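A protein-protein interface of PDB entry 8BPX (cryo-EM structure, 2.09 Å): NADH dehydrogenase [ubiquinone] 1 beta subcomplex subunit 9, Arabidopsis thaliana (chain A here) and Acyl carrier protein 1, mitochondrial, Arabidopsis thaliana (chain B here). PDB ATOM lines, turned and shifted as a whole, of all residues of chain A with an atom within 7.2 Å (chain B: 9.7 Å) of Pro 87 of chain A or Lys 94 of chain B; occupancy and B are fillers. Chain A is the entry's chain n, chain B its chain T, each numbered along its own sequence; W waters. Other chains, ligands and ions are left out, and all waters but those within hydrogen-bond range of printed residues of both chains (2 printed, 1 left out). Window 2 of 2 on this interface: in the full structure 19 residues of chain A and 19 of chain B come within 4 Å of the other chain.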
ATOM      1  N   TYR A  84       0.058 -10.456  20.938  1.00  0.00           N
ATOM      2  CA  TYR A  84       1.056  -9.609  20.306  1.00  0.00           C
ATOM      3  C   TYR A  84       1.012  -8.203  20.891  1.00  0.00           C
ATOM      4  O   TYR A  84      -0.060  -7.645  21.129  1.00  0.00           O
ATOM      5  CB  TYR A  84       0.833  -9.536  18.794  1.00  0.00           C
ATOM      6  CG  TYR A  84       1.686  -8.474  18.155  1.00  0.00           C
ATOM      7  CD1 TYR A  84       3.036  -8.697  17.916  1.00  0.00           C
ATOM      8  CD2 TYR A  84       1.162  -7.225  17.844  1.00  0.00           C
ATOM      9  CE1 TYR A  84       3.829  -7.720  17.363  1.00  0.00           C
ATOM     10  CE2 TYR A  84       1.951  -6.240  17.294  1.00  0.00           C
ATOM     11  CZ  TYR A  84       3.283  -6.493  17.054  1.00  0.00           C
ATOM     12  OH  TYR A  84       4.070  -5.519  16.499  1.00  0.00           O
ATOM     13  N   ILE A  85       2.186  -7.624  21.111  1.00  0.00           N
ATOM     14  CA  ILE A  85       2.305  -6.240  21.553  1.00  0.00           C
ATOM     15  C   ILE A  85       3.362  -5.549  20.706  1.00  0.00           C
ATOM     16  O   ILE A  85       4.438  -6.106  20.471  1.00  0.00           O
ATOM     17  CB  ILE A  85       2.658  -6.131  23.054  1.00  0.00           C
ATOM     18  CG1 ILE A  85       1.639  -6.874  23.916  1.00  0.00           C
ATOM     19  CG2 ILE A  85       2.755  -4.671  23.487  1.00  0.00           C
ATOM     20  CD1 ILE A  85       2.252  -7.673  25.036  1.00  0.00           C
ATOM     21  N   VAL A  86       3.053  -4.340  20.253  1.00  0.00           N
ATOM     22  CA  VAL A  86       4.061  -3.504  19.592  1.00  0.00           C
ATOM     23  C   VAL A  86       5.251  -3.325  20.532  1.00  0.00           C
ATOM     24  O   VAL A  86       5.053  -3.065  21.733  1.00  0.00           O
ATOM     25  CB  VAL A  86       3.454  -2.145  19.196  1.00  0.00           C
ATOM     26  CG1 VAL A  86       4.456  -1.289  18.448  1.00  0.00           C
ATOM     27  CG2 VAL A  86       2.203  -2.353  18.354  1.00  0.00           C
ATOM     28  N   PRO A  87       6.490  -3.467  20.050  1.00  0.00           N
ATOM     29  CA  PRO A  87       7.635  -3.554  20.976  1.00  0.00           C
ATOM     30  C   PRO A  87       7.799  -2.366  21.914  1.00  0.00           C
ATOM     31  O   PRO A  87       8.261  -2.552  23.044  1.00  0.00           O
ATOM     32  CB  PRO A  87       8.832  -3.695  20.026  1.00  0.00           C
ATOM     33  CG  PRO A  87       8.266  -4.282  18.795  1.00  0.00           C
ATOM     34  CD  PRO A  87       6.887  -3.725  18.655  1.00  0.00           C
ATOM     35  N   TRP A  88       7.440  -1.154  21.494  1.00  0.00           N
ATOM     36  CA  TRP A  88       7.596   0.012  22.356  1.00  0.00           C
ATOM     37  C   TRP A  88       6.374   0.296  23.224  1.00  0.00           C
ATOM     38  O   TRP A  88       6.428   1.200  24.059  1.00  0.00           O
ATOM     39  CB  TRP A  88       7.943   1.252  21.522  1.00  0.00           C
ATOM     40  CG  TRP A  88       7.089   1.453  20.321  1.00  0.00           C
ATOM     41  CD1 TRP A  88       7.404   1.139  19.034  1.00  0.00           C
ATOM     42  CD2 TRP A  88       5.773   2.013  20.284  1.00  0.00           C
ATOM     43  NE1 TRP A  88       6.370   1.469  18.197  1.00  0.00           N
ATOM     44  CE2 TRP A  88       5.355   2.005  18.941  1.00  0.00           C
ATOM     45  CE3 TRP A  88       4.906   2.514  21.259  1.00  0.00           C
ATOM     46  CZ2 TRP A  88       4.108   2.483  18.546  1.00  0.00           C
ATOM     47  CZ3 TRP A  88       3.668   2.986  20.865  1.00  0.00           C
ATOM     48  CH2 TRP A  88       3.281   2.966  19.521  1.00  0.00           C
ATOM     49  N   ALA A  89       5.288  -0.444  23.052  1.00  0.00           N
ATOM     50  CA  ALA A  89       4.106  -0.288  23.884  1.00  0.00           C
ATOM     51  C   ALA A  89       4.326  -0.936  25.250  1.00  0.00           C
ATOM     52  O   ALA A  89       5.229  -1.758  25.415  1.00  0.00           O
ATOM     53  CB  ALA A  89       2.897  -0.897  23.185  1.00  0.00           C
ATOM     54  N   PRO A  90       3.538  -0.556  26.256  1.00  0.00           N
ATOM     55  CA  PRO A  90       3.687  -1.182  27.578  1.00  0.00           C
ATOM     56  C   PRO A  90       3.516  -2.692  27.505  1.00  0.00           C
ATOM     57  O   PRO A  90       2.558  -3.200  26.922  1.00  0.00           O
ATOM     58  CB  PRO A  90       2.584  -0.521  28.416  1.00  0.00           C
ATOM     59  CG  PRO A  90       1.711   0.189  27.448  1.00  0.00           C
ATOM     60  CD  PRO A  90       2.556   0.540  26.282  1.00  0.00           C
ATOM     61  N   GLY A  91       4.457  -3.408  28.115  1.00  0.00           N
ATOM     62  CA  GLY A  91       4.544  -4.843  27.974  1.00  0.00           C
ATOM     63  C   GLY A  91       5.344  -5.311  26.779  1.00  0.00           C
ATOM     64  O   GLY A  91       5.590  -6.516  26.654  1.00  0.00           O
ATOM     65  N   GLY A  92       5.770  -4.398  25.904  1.00  0.00           N
ATOM     66  CA  GLY A  92       6.513  -4.771  24.723  1.00  0.00           C
ATOM     67  C   GLY A  92       7.967  -5.089  25.009  1.00  0.00           C
ATOM     68  O   GLY A  92       8.506  -4.808  26.077  1.00  0.00           O
ATOM     69  N   SER A  93       8.617  -5.685  24.006  1.00  0.00           N
ATOM     70  CA  SER A  93      10.003  -6.102  24.164  1.00  0.00           C
ATOM     71  C   SER A  93      10.966  -4.922  24.232  1.00  0.00           C
ATOM     72  O   SER A  93      12.037  -5.051  24.831  1.00  0.00           O
ATOM     73  CB  SER A  93      10.393  -7.047  23.024  1.00  0.00           C
ATOM     74  OG  SER A  93      10.389  -6.378  21.778  1.00  0.00           O
ATOM     75  N   LYS A  94      10.608  -3.780  23.646  1.00  0.00           N
ATOM     76  CA  LYS A  94      11.432  -2.576  23.667  1.00  0.00           C
ATOM     77  C   LYS A  94      10.984  -1.550  24.704  1.00  0.00           C
ATOM     78  O   LYS A  94      11.565  -0.463  24.771  1.00  0.00           O
ATOM     79  CB  LYS A  94      11.446  -1.921  22.287  1.00  0.00           C
ATOM     80  CG  LYS A  94      12.823  -1.633  21.750  1.00  0.00           C
ATOM     81  CD  LYS A  94      12.782  -0.476  20.779  1.00  0.00           C
ATOM     82  CE  LYS A  94      14.090  -0.317  20.046  1.00  0.00           C
ATOM     83  NZ  LYS A  94      13.938   0.523  18.831  1.00  0.00           N
ATOM     84  N   PHE A  95       9.972  -1.860  25.508  1.00  0.00           N
ATOM     85  CA  PHE A  95       9.397  -0.874  26.415  1.00  0.00           C
ATOM     86  C   PHE A  95      10.390  -0.505  27.514  1.00  0.00           C
ATOM     87  O   PHE A  95      10.946  -1.380  28.184  1.00  0.00           O
ATOM     88  CB  PHE A  95       8.100  -1.419  27.015  1.00  0.00           C
ATOM     89  CG  PHE A  95       7.299  -0.397  27.773  1.00  0.00           C
ATOM     90  CD1 PHE A  95       6.982   0.824  27.199  1.00  0.00           C
ATOM     91  CD2 PHE A  95       6.852  -0.661  29.056  1.00  0.00           C
ATOM     92  CE1 PHE A  95       6.244   1.768  27.895  1.00  0.00           C
ATOM     93  CE2 PHE A  95       6.110   0.281  29.759  1.00  0.00           C
ATOM     94  CZ  PHE A  95       5.809   1.495  29.176  1.00  0.00           C
ATOM     95  N   CYS A  96      10.613   0.802  27.687  1.00  0.00           N
ATOM     96  CA  CYS A  96      11.498   1.365  28.715  1.00  0.00           C
ATOM     97  C   CYS A  96      12.969   0.997  28.507  1.00  0.00           C
ATOM     98  O   CYS A  96      13.730   0.930  29.473  1.00  0.00           O
ATOM     99  CB  CYS A  96      11.056   0.951  30.124  1.00  0.00           C
ATOM    100  SG  CYS A  96       9.315   1.232  30.512  1.00  0.00           S
ATOM    101  N   ARG B  49      -2.558   9.311   4.175  1.00  0.00           N
ATOM    102  CA  ARG B  49      -2.656   7.878   4.500  1.00  0.00           C
ATOM    103  C   ARG B  49      -3.890   7.558   5.390  1.00  0.00           C
ATOM    104  O   ARG B  49      -4.394   6.460   5.280  1.00  0.00           O
ATOM    105  CB  ARG B  49      -1.329   7.381   5.096  1.00  0.00           C
ATOM    106  CG  ARG B  49      -0.060   7.576   4.298  1.00  0.00           C
ATOM    107  CD  ARG B  49       0.825   6.610   5.045  1.00  0.00           C
ATOM    108  NE  ARG B  49       1.946   7.134   5.799  1.00  0.00           N
ATOM    109  CZ  ARG B  49       2.550   6.481   6.776  1.00  0.00           C
ATOM    110  NH1 ARG B  49       2.103   5.301   7.171  1.00  0.00           N
ATOM    111  NH2 ARG B  49       3.571   7.034   7.398  1.00  0.00           N
ATOM    112  N   VAL B  53      -6.910   5.055   4.180  1.00  0.00           N
ATOM    113  CA  VAL B  53      -7.449   3.967   4.991  1.00  0.00           C
ATOM    114  C   VAL B  53      -8.972   4.031   5.017  1.00  0.00           C
ATOM    115  O   VAL B  53      -9.659   3.024   4.800  1.00  0.00           O
ATOM    116  CB  VAL B  53      -6.863   4.003   6.414  1.00  0.00           C
ATOM    117  CG1 VAL B  53      -7.661   3.094   7.332  1.00  0.00           C
ATOM    118  CG2 VAL B  53      -5.400   3.593   6.406  1.00  0.00           C
ATOM    119  N   VAL B  86     -10.515   2.180  12.975  1.00  0.00           N
ATOM    120  CA  VAL B  86      -9.465   2.549  13.920  1.00  0.00           C
ATOM    121  C   VAL B  86      -8.399   1.462  13.983  1.00  0.00           C
ATOM    122  O   VAL B  86      -7.201   1.756  14.020  1.00  0.00           O
ATOM    123  CB  VAL B  86     -10.068   2.853  15.304  1.00  0.00           C
ATOM    124  CG1 VAL B  86      -8.973   2.985  16.354  1.00  0.00           C
ATOM    125  CG2 VAL B  86     -10.899   4.122  15.246  1.00  0.00           C
ATOM    126  N   MET B  87      -8.800   0.175  14.007  1.00  0.00           N
ATOM    127  CA  MET B  87      -7.831  -0.957  13.941  1.00  0.00           C
ATOM    128  C   MET B  87      -7.010  -0.881  12.636  1.00  0.00           C
ATOM    129  O   MET B  87      -5.836  -1.114  12.700  1.00  0.00           O
ATOM    130  CB  MET B  87      -8.483  -2.339  14.107  1.00  0.00           C
ATOM    131  CG  MET B  87      -7.494  -3.506  14.064  1.00  0.00           C
ATOM    132  SD  MET B  87      -8.109  -5.185  14.428  1.00  0.00           S
ATOM    133  CE  MET B  87      -6.654  -6.171  14.084  1.00  0.00           C
ATOM    134  N   ALA B  88      -7.632  -0.488  11.534  1.00  0.00           N
ATOM    135  CA  ALA B  88      -6.896  -0.380  10.277  1.00  0.00           C
ATOM    136  C   ALA B  88      -5.882   0.759  10.320  1.00  0.00           C
ATOM    137  O   ALA B  88      -4.768   0.624   9.806  1.00  0.00           O
ATOM    138  CB  ALA B  88      -7.864  -0.196   9.114  1.00  0.00           C
ATOM    139  N   ILE B  89      -6.250   1.889  10.926  1.00  0.00           N
ATOM    140  CA  ILE B  89      -5.304   2.993  11.106  1.00  0.00           C
ATOM    141  C   ILE B  89      -4.148   2.557  12.002  1.00  0.00           C
ATOM    142  O   ILE B  89      -2.975   2.876  11.746  1.00  0.00           O
ATOM    143  CB  ILE B  89      -6.033   4.226  11.670  1.00  0.00           C
ATOM    144  CG1 ILE B  89      -6.905   4.873  10.593  1.00  0.00           C
ATOM    145  CG2 ILE B  89      -5.047   5.241  12.233  1.00  0.00           C
ATOM    146  CD1 ILE B  89      -8.056   5.694  11.145  1.00  0.00           C
ATOM    147  N   GLU B  90      -4.471   1.824  13.073  1.00  0.00           N
ATOM    148  CA  GLU B  90      -3.464   1.254  13.961  1.00  0.00           C
ATOM    149  C   GLU B  90      -2.448   0.432  13.180  1.00  0.00           C
ATOM    150  O   GLU B  90      -1.235   0.600  13.343  1.00  0.00           O
ATOM    151  CB  GLU B  90      -4.147   0.373  15.009  1.00  0.00           C
ATOM    152  CG  GLU B  90      -4.756   1.095  16.191  1.00  0.00           C
ATOM    153  CD  GLU B  90      -3.736   1.393  17.258  1.00  0.00           C
ATOM    154  OE1 GLU B  90      -2.843   2.219  16.995  1.00  0.00           O
ATOM    155  OE2 GLU B  90      -3.823   0.808  18.357  1.00  0.00           O
ATOM    156  N   GLU B  91      -2.863  -0.395  12.205  1.00  0.00           N
ATOM    157  CA  GLU B  91      -1.952  -1.288  11.467  1.00  0.00           C
ATOM    158  C   GLU B  91      -1.217  -0.415  10.473  1.00  0.00           C
ATOM    159  O   GLU B  91      -0.052  -0.635  10.238  1.00  0.00           O
ATOM    160  CB  GLU B  91      -2.672  -2.436  10.737  1.00  0.00           C
ATOM    161  CG  GLU B  91      -3.131  -3.572  11.620  1.00  0.00           C
ATOM    162  CD  GLU B  91      -3.389  -4.859  10.848  1.00  0.00           C
ATOM    163  OE1 GLU B  91      -3.924  -5.813  11.438  1.00  0.00           O
ATOM    164  OE2 GLU B  91      -3.036  -4.904   9.654  1.00  0.00           O
ATOM    165  N   GLU B  92      -1.910   0.573   9.983  1.00  0.00           N
ATOM    166  CA  GLU B  92      -1.281   1.356   8.931  1.00  0.00           C
ATOM    167  C   GLU B  92      -0.088   2.144   9.459  1.00  0.00           C
ATOM    168  O   GLU B  92       0.916   2.298   8.755  1.00  0.00           O
ATOM    169  CB  GLU B  92      -2.311   2.286   8.290  1.00  0.00           C
ATOM    170  CG  GLU B  92      -1.703   3.439   7.532  1.00  0.00           C
ATOM    171  CD  GLU B  92      -1.097   2.979   6.228  1.00  0.00           C
ATOM    172  OE1 GLU B  92      -1.333   1.819   5.832  1.00  0.00           O
ATOM    173  OE2 GLU B  92      -0.370   3.763   5.599  1.00  0.00           O
ATOM    174  N   PHE B  93      -0.105   2.632  10.714  1.00  0.00           N
ATOM    175  CA  PHE B  93       1.025   3.438  11.242  1.00  0.00           C
ATOM    176  C   PHE B  93       1.831   2.620  12.268  1.00  0.00           C
ATOM    177  O   PHE B  93       2.766   3.206  12.795  1.00  0.00           O
ATOM    178  CB  PHE B  93       0.543   4.811  11.782  1.00  0.00           C
ATOM    179  CG  PHE B  93       0.052   5.779  10.738  1.00  0.00           C
ATOM    180  CD1 PHE B  93       0.936   6.602  10.063  1.00  0.00           C
ATOM    181  CD2 PHE B  93      -1.294   5.870  10.431  1.00  0.00           C
ATOM    182  CE1 PHE B  93       0.484   7.499   9.112  1.00  0.00           C
ATOM    183  CE2 PHE B  93      -1.745   6.759   9.471  1.00  0.00           C
ATOM    184  CZ  PHE B  93      -0.854   7.574   8.816  1.00  0.00           C
ATOM    185  N   LYS B  94       1.488   1.334  12.533  1.00  0.00           N
ATOM    186  CA  LYS B  94       2.162   0.519  13.598  1.00  0.00           C
ATOM    187  C   LYS B  94       2.039   1.222  14.965  1.00  0.00           C
ATOM    188  O   LYS B  94       3.033   1.402  15.620  1.00  0.00           O
ATOM    189  CB  LYS B  94       3.567  -0.015  13.258  1.00  0.00           C
ATOM    190  CG  LYS B  94       3.946  -1.270  14.023  1.00  0.00           C
ATOM    191  CD  LYS B  94       5.390  -1.705  13.966  1.00  0.00           C
ATOM    192  CE  LYS B  94       5.599  -2.968  14.783  1.00  0.00           C
ATOM    193  NZ  LYS B  94       6.986  -3.484  14.738  1.00  0.00           N
ATOM    194  N   LEU B  95       0.823   1.424  15.432  1.00  0.00           N
ATOM    195  CA  LEU B  95       0.648   1.999  16.755  1.00  0.00           C
ATOM    196  C   LEU B  95      -0.190   1.061  17.609  1.00  0.00           C
ATOM    197  O   LEU B  95      -0.902   0.191  17.102  1.00  0.00           O
ATOM    198  CB  LEU B  95      -0.009   3.384  16.702  1.00  0.00           C
ATOM    199  CG  LEU B  95       0.506   4.368  15.656  1.00  0.00           C
ATOM    200  CD1 LEU B  95      -0.505   5.483  15.419  1.00  0.00           C
ATOM    201  CD2 LEU B  95       1.863   4.918  16.037  1.00  0.00           C
ATOM    202  N   GLU B  96      -0.085   1.234  18.920  1.00  0.00           N
ATOM    203  CA  GLU B  96      -0.909   0.504  19.880  1.00  0.00           C
ATOM    204  C   GLU B  96      -1.646   1.546  20.715  1.00  0.00           C
ATOM    205  O   GLU B  96      -1.137   2.000  21.743  1.00  0.00           O
ATOM    206  CB  GLU B  96      -0.070  -0.430  20.748  1.00  0.00           C
ATOM    207  CG  GLU B  96      -0.890  -1.426  21.549  1.00  0.00           C
ATOM    208  CD  GLU B  96      -0.202  -2.776  21.709  1.00  0.00           C
ATOM    209  OE1 GLU B  96       0.347  -3.286  20.715  1.00  0.00           O
ATOM    210  OE2 GLU B  96      -0.219  -3.332  22.824  1.00  0.00           O
ATOM    211  N   ILE B  97      -2.826   1.935  20.260  1.00  0.00           N
ATOM    212  CA  ILE B  97      -3.630   2.926  20.977  1.00  0.00           C
ATOM    213  C   ILE B  97      -4.290   2.252  22.177  1.00  0.00           C
ATOM    214  O   ILE B  97      -4.836   1.149  22.035  1.00  0.00           O
ATOM    215  CB  ILE B  97      -4.672   3.542  20.051  1.00  0.00           C
ATOM    216  CG1 ILE B  97      -3.983   4.305  18.925  1.00  0.00           C
ATOM    217  CG2 ILE B  97      -5.583   4.484  20.825  1.00  0.00           C
ATOM    218  CD1 ILE B  97      -4.875   4.627  17.757  1.00  0.00           C
ATOM    219  N   TYR B 114      -4.523  12.398  16.346  1.00  0.00           N
ATOM    220  CA  TYR B 114      -3.850  11.414  17.188  1.00  0.00           C
ATOM    221  C   TYR B 114      -2.588  10.882  16.519  1.00  0.00           C
ATOM    222  O   TYR B 114      -1.534  10.779  17.156  1.00  0.00           O
ATOM    223  CB  TYR B 114      -4.798  10.267  17.535  1.00  0.00           C
ATOM    224  CG  TYR B 114      -4.205   9.301  18.530  1.00  0.00           C
ATOM    225  CD1 TYR B 114      -3.344   8.294  18.121  1.00  0.00           C
ATOM    226  CD2 TYR B 114      -4.485   9.411  19.883  1.00  0.00           C
ATOM    227  CE1 TYR B 114      -2.784   7.428  19.023  1.00  0.00           C
ATOM    228  CE2 TYR B 114      -3.932   8.538  20.794  1.00  0.00           C
ATOM    229  CZ  TYR B 114      -3.085   7.548  20.358  1.00  0.00           C
ATOM    230  OH  TYR B 114      -2.531   6.672  21.258  1.00  0.00           O
ATOM    231  N   VAL B 115      -2.674  10.539  15.232  1.00  0.00           N
ATOM    232  CA  VAL B 115      -1.518   9.966  14.548  1.00  0.00           C
ATOM    233  C   VAL B 115      -0.411  11.002  14.399  1.00  0.00           C
ATOM    234  O   VAL B 115       0.768  10.703  14.621  1.00  0.00           O
ATOM    235  CB  VAL B 115      -1.938   9.372  13.192  1.00  0.00           C
ATOM    236  CG1 VAL B 115      -0.717   8.968  12.374  1.00  0.00           C
ATOM    237  CG2 VAL B 115      -2.844   8.171  13.409  1.00  0.00           C
ATOM    238  N   HIS B 118       1.302  11.583  17.764  1.00  0.00           N
ATOM    239  CA  HIS B 118       2.030  10.464  18.341  1.00  0.00           C
ATOM    240  C   HIS B 118       3.475  10.503  17.861  1.00  0.00           C
ATOM    241  O   HIS B 118       3.722  10.536  16.652  1.00  0.00           O
ATOM    242  CB  HIS B 118       1.392   9.127  17.980  1.00  0.00           C
ATOM    243  CG  HIS B 118       1.708   8.042  18.958  1.00  0.00           C
ATOM    244  ND1 HIS B 118       2.062   8.304  20.261  1.00  0.00           N
ATOM    245  CD2 HIS B 118       1.774   6.699  18.816  1.00  0.00           C
ATOM    246  CE1 HIS B 118       2.308   7.168  20.888  1.00  0.00           C
ATOM    247  NE2 HIS B 118       2.144   6.180  20.032  1.00  0.00           N
ATOM    248  N   PRO B 119       4.452  10.520  18.769  1.00  0.00           N
ATOM    249  CA  PRO B 119       5.855  10.588  18.337  1.00  0.00           C
ATOM    250  C   PRO B 119       6.365   9.328  17.664  1.00  0.00           C
ATOM    251  O   PRO B 119       7.370   9.399  16.948  1.00  0.00           O
ATOM    252  CB  PRO B 119       6.611  10.849  19.646  1.00  0.00           C
ATOM    253  CG  PRO B 119       5.736  10.294  20.693  1.00  0.00           C
ATOM    254  CD  PRO B 119       4.327  10.501  20.235  1.00  0.00           C
ATOM    255  N   MET B 120       5.725   8.185  17.866  1.00  0.00           N
ATOM    256  CA  MET B 120       6.217   6.943  17.293  1.00  0.00           C
ATOM    257  C   MET B 120       5.521   6.576  15.991  1.00  0.00           C
ATOM    258  O   MET B 120       5.757   5.485  15.467  1.00  0.00           O
ATOM    259  CB  MET B 120       6.076   5.800  18.297  1.00  0.00           C
ATOM    260  CG  MET B 120       7.113   5.838  19.400  1.00  0.00           C
ATOM    261  SD  MET B 120       8.735   5.252  18.890  1.00  0.00           S
ATOM    262  CE  MET B 120       8.320   3.997  17.689  1.00  0.00           C
ATOM    263  N   SER B 121       4.697   7.444  15.414  1.00  0.00           N
ATOM    264  CA  SER B 121       4.044   7.133  14.108  1.00  0.00           C
ATOM    265  C   SER B 121       5.040   7.148  12.939  1.00  0.00           C
ATOM    266  O   SER B 121       4.844   6.376  11.989  1.00  0.00           O
ATOM    267  CB  SER B 121       2.897   8.066  13.858  1.00  0.00           C
ATOM    268  OG  SER B 121       2.000   8.082  14.956  1.00  0.00           O
HETATM  269  O   HOH W   1      -0.991  -5.669  22.735  1.00  0.00           O
HETATM  270  O   HOH W   2       0.762  -2.220  25.392  1.00  0.00           O
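Water W1 lies within hydrogen-bond range of the side-chain carboxylate (OE2) of Glu 96 of chain B and the backbone carbonyl oxygen (O) of Tyr 84 of chain A.
Water W2 bridges the backbone carbonyl oxygen of Pro 90 of chain A (2.6 Å) and the side-chain carboxylate of Glu 96 of chain B (3.0 Å).
Of the printed residues of chain B, Ile 85 of chain A touches Glu 96.
Val 86 of chain A touches just one residue of chain B: Glu 96 (2.9 Å).
Of the printed residues of chain B, Trp 88 of chain A touches Lys 94 (3.3 Å), Leu 95 (3.9 Å), Glu 96 (3.8 Å), His 118 (3.4 Å) and Met 120 (3.2 Å).
No residue of chain B comes within 4 Å of Ser 93 of chain A.
Arg 49 of chain B touches none of the printed residues of chain A.
Ile 89 of chain B touches none of the printed residues of chain A.
Printed residues of chain A within 4 Å of Met 120 of chain B: Trp 88 (3.2 Å).
The nearest residue of chain B that does not touch Pro 87 of chain A is Glu 96 of chain B (6.2 Å).
Hydrophobic or aromatic side chains of chain A that line the printed part of chain B: Tyr 84, Ile 85, Val 86, Pro 87, Trp 88 and Ala 89.
Hydrophobic or aromatic side chains of chain B within 4 Å of the printed part of chain A: His 118 and Met 120.
Along chain B the printed residues that touch a printed residue of chain A span positions 94 to 120.
Among the printed residues, 10 pairs touch across the chains.
N of Leu 95 of chain B sits at hydrogen-bond distance from O of Glu 90 of chain B (3.0 Å).
The side-chain hydroxyl of Ser 121 of chain B lies close to the backbone carbonyl oxygen of His 118 of chain B (3.4 Å).
The backbone NH (N) of Ser 93 of chain A lies within hydrogen-bond range of the backbone carbonyl oxygen (O) of Pro 87 of chain A, 3.3 Å away.
O of Pro 87 of chain A is in hydrogen-bond range of N of Lys 94 of chain A (2.7 Å).
O of Pro 87 of chain A is in hydrogen-bond range of N of Phe 95 of chain A (3.1 Å).
The side-chain carboxylate of Glu 96 of chain B sits at hydrogen-bond distance from the backbone NH of Val 86 of chain A, at 2.9 Å.
Among the printed residues, pairs that only touch across the chains: Trp 88 of chain A with Met 120 of chain B (3.2 Å), Trp 88 of chain A with Lys 94 of chain B (3.3 Å), Ile 85 of chain A with Glu 96 of chain B (3.3 Å), Tyr 84 of chain A with Lys 94 of chain B (3.4 Å), Trp 88 of chain A with His 118 of chain B (3.4 Å), Trp 88 of chain A with Glu 96 of chain B (3.8 Å), Ala 89 of chain A with Glu 96 of chain B (3.9 Å), Pro 87 of chain A with Lys 94 of chain B (3.9 Å) and Trp 88 of chain A with Leu 95 of chain B (3.9 Å).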
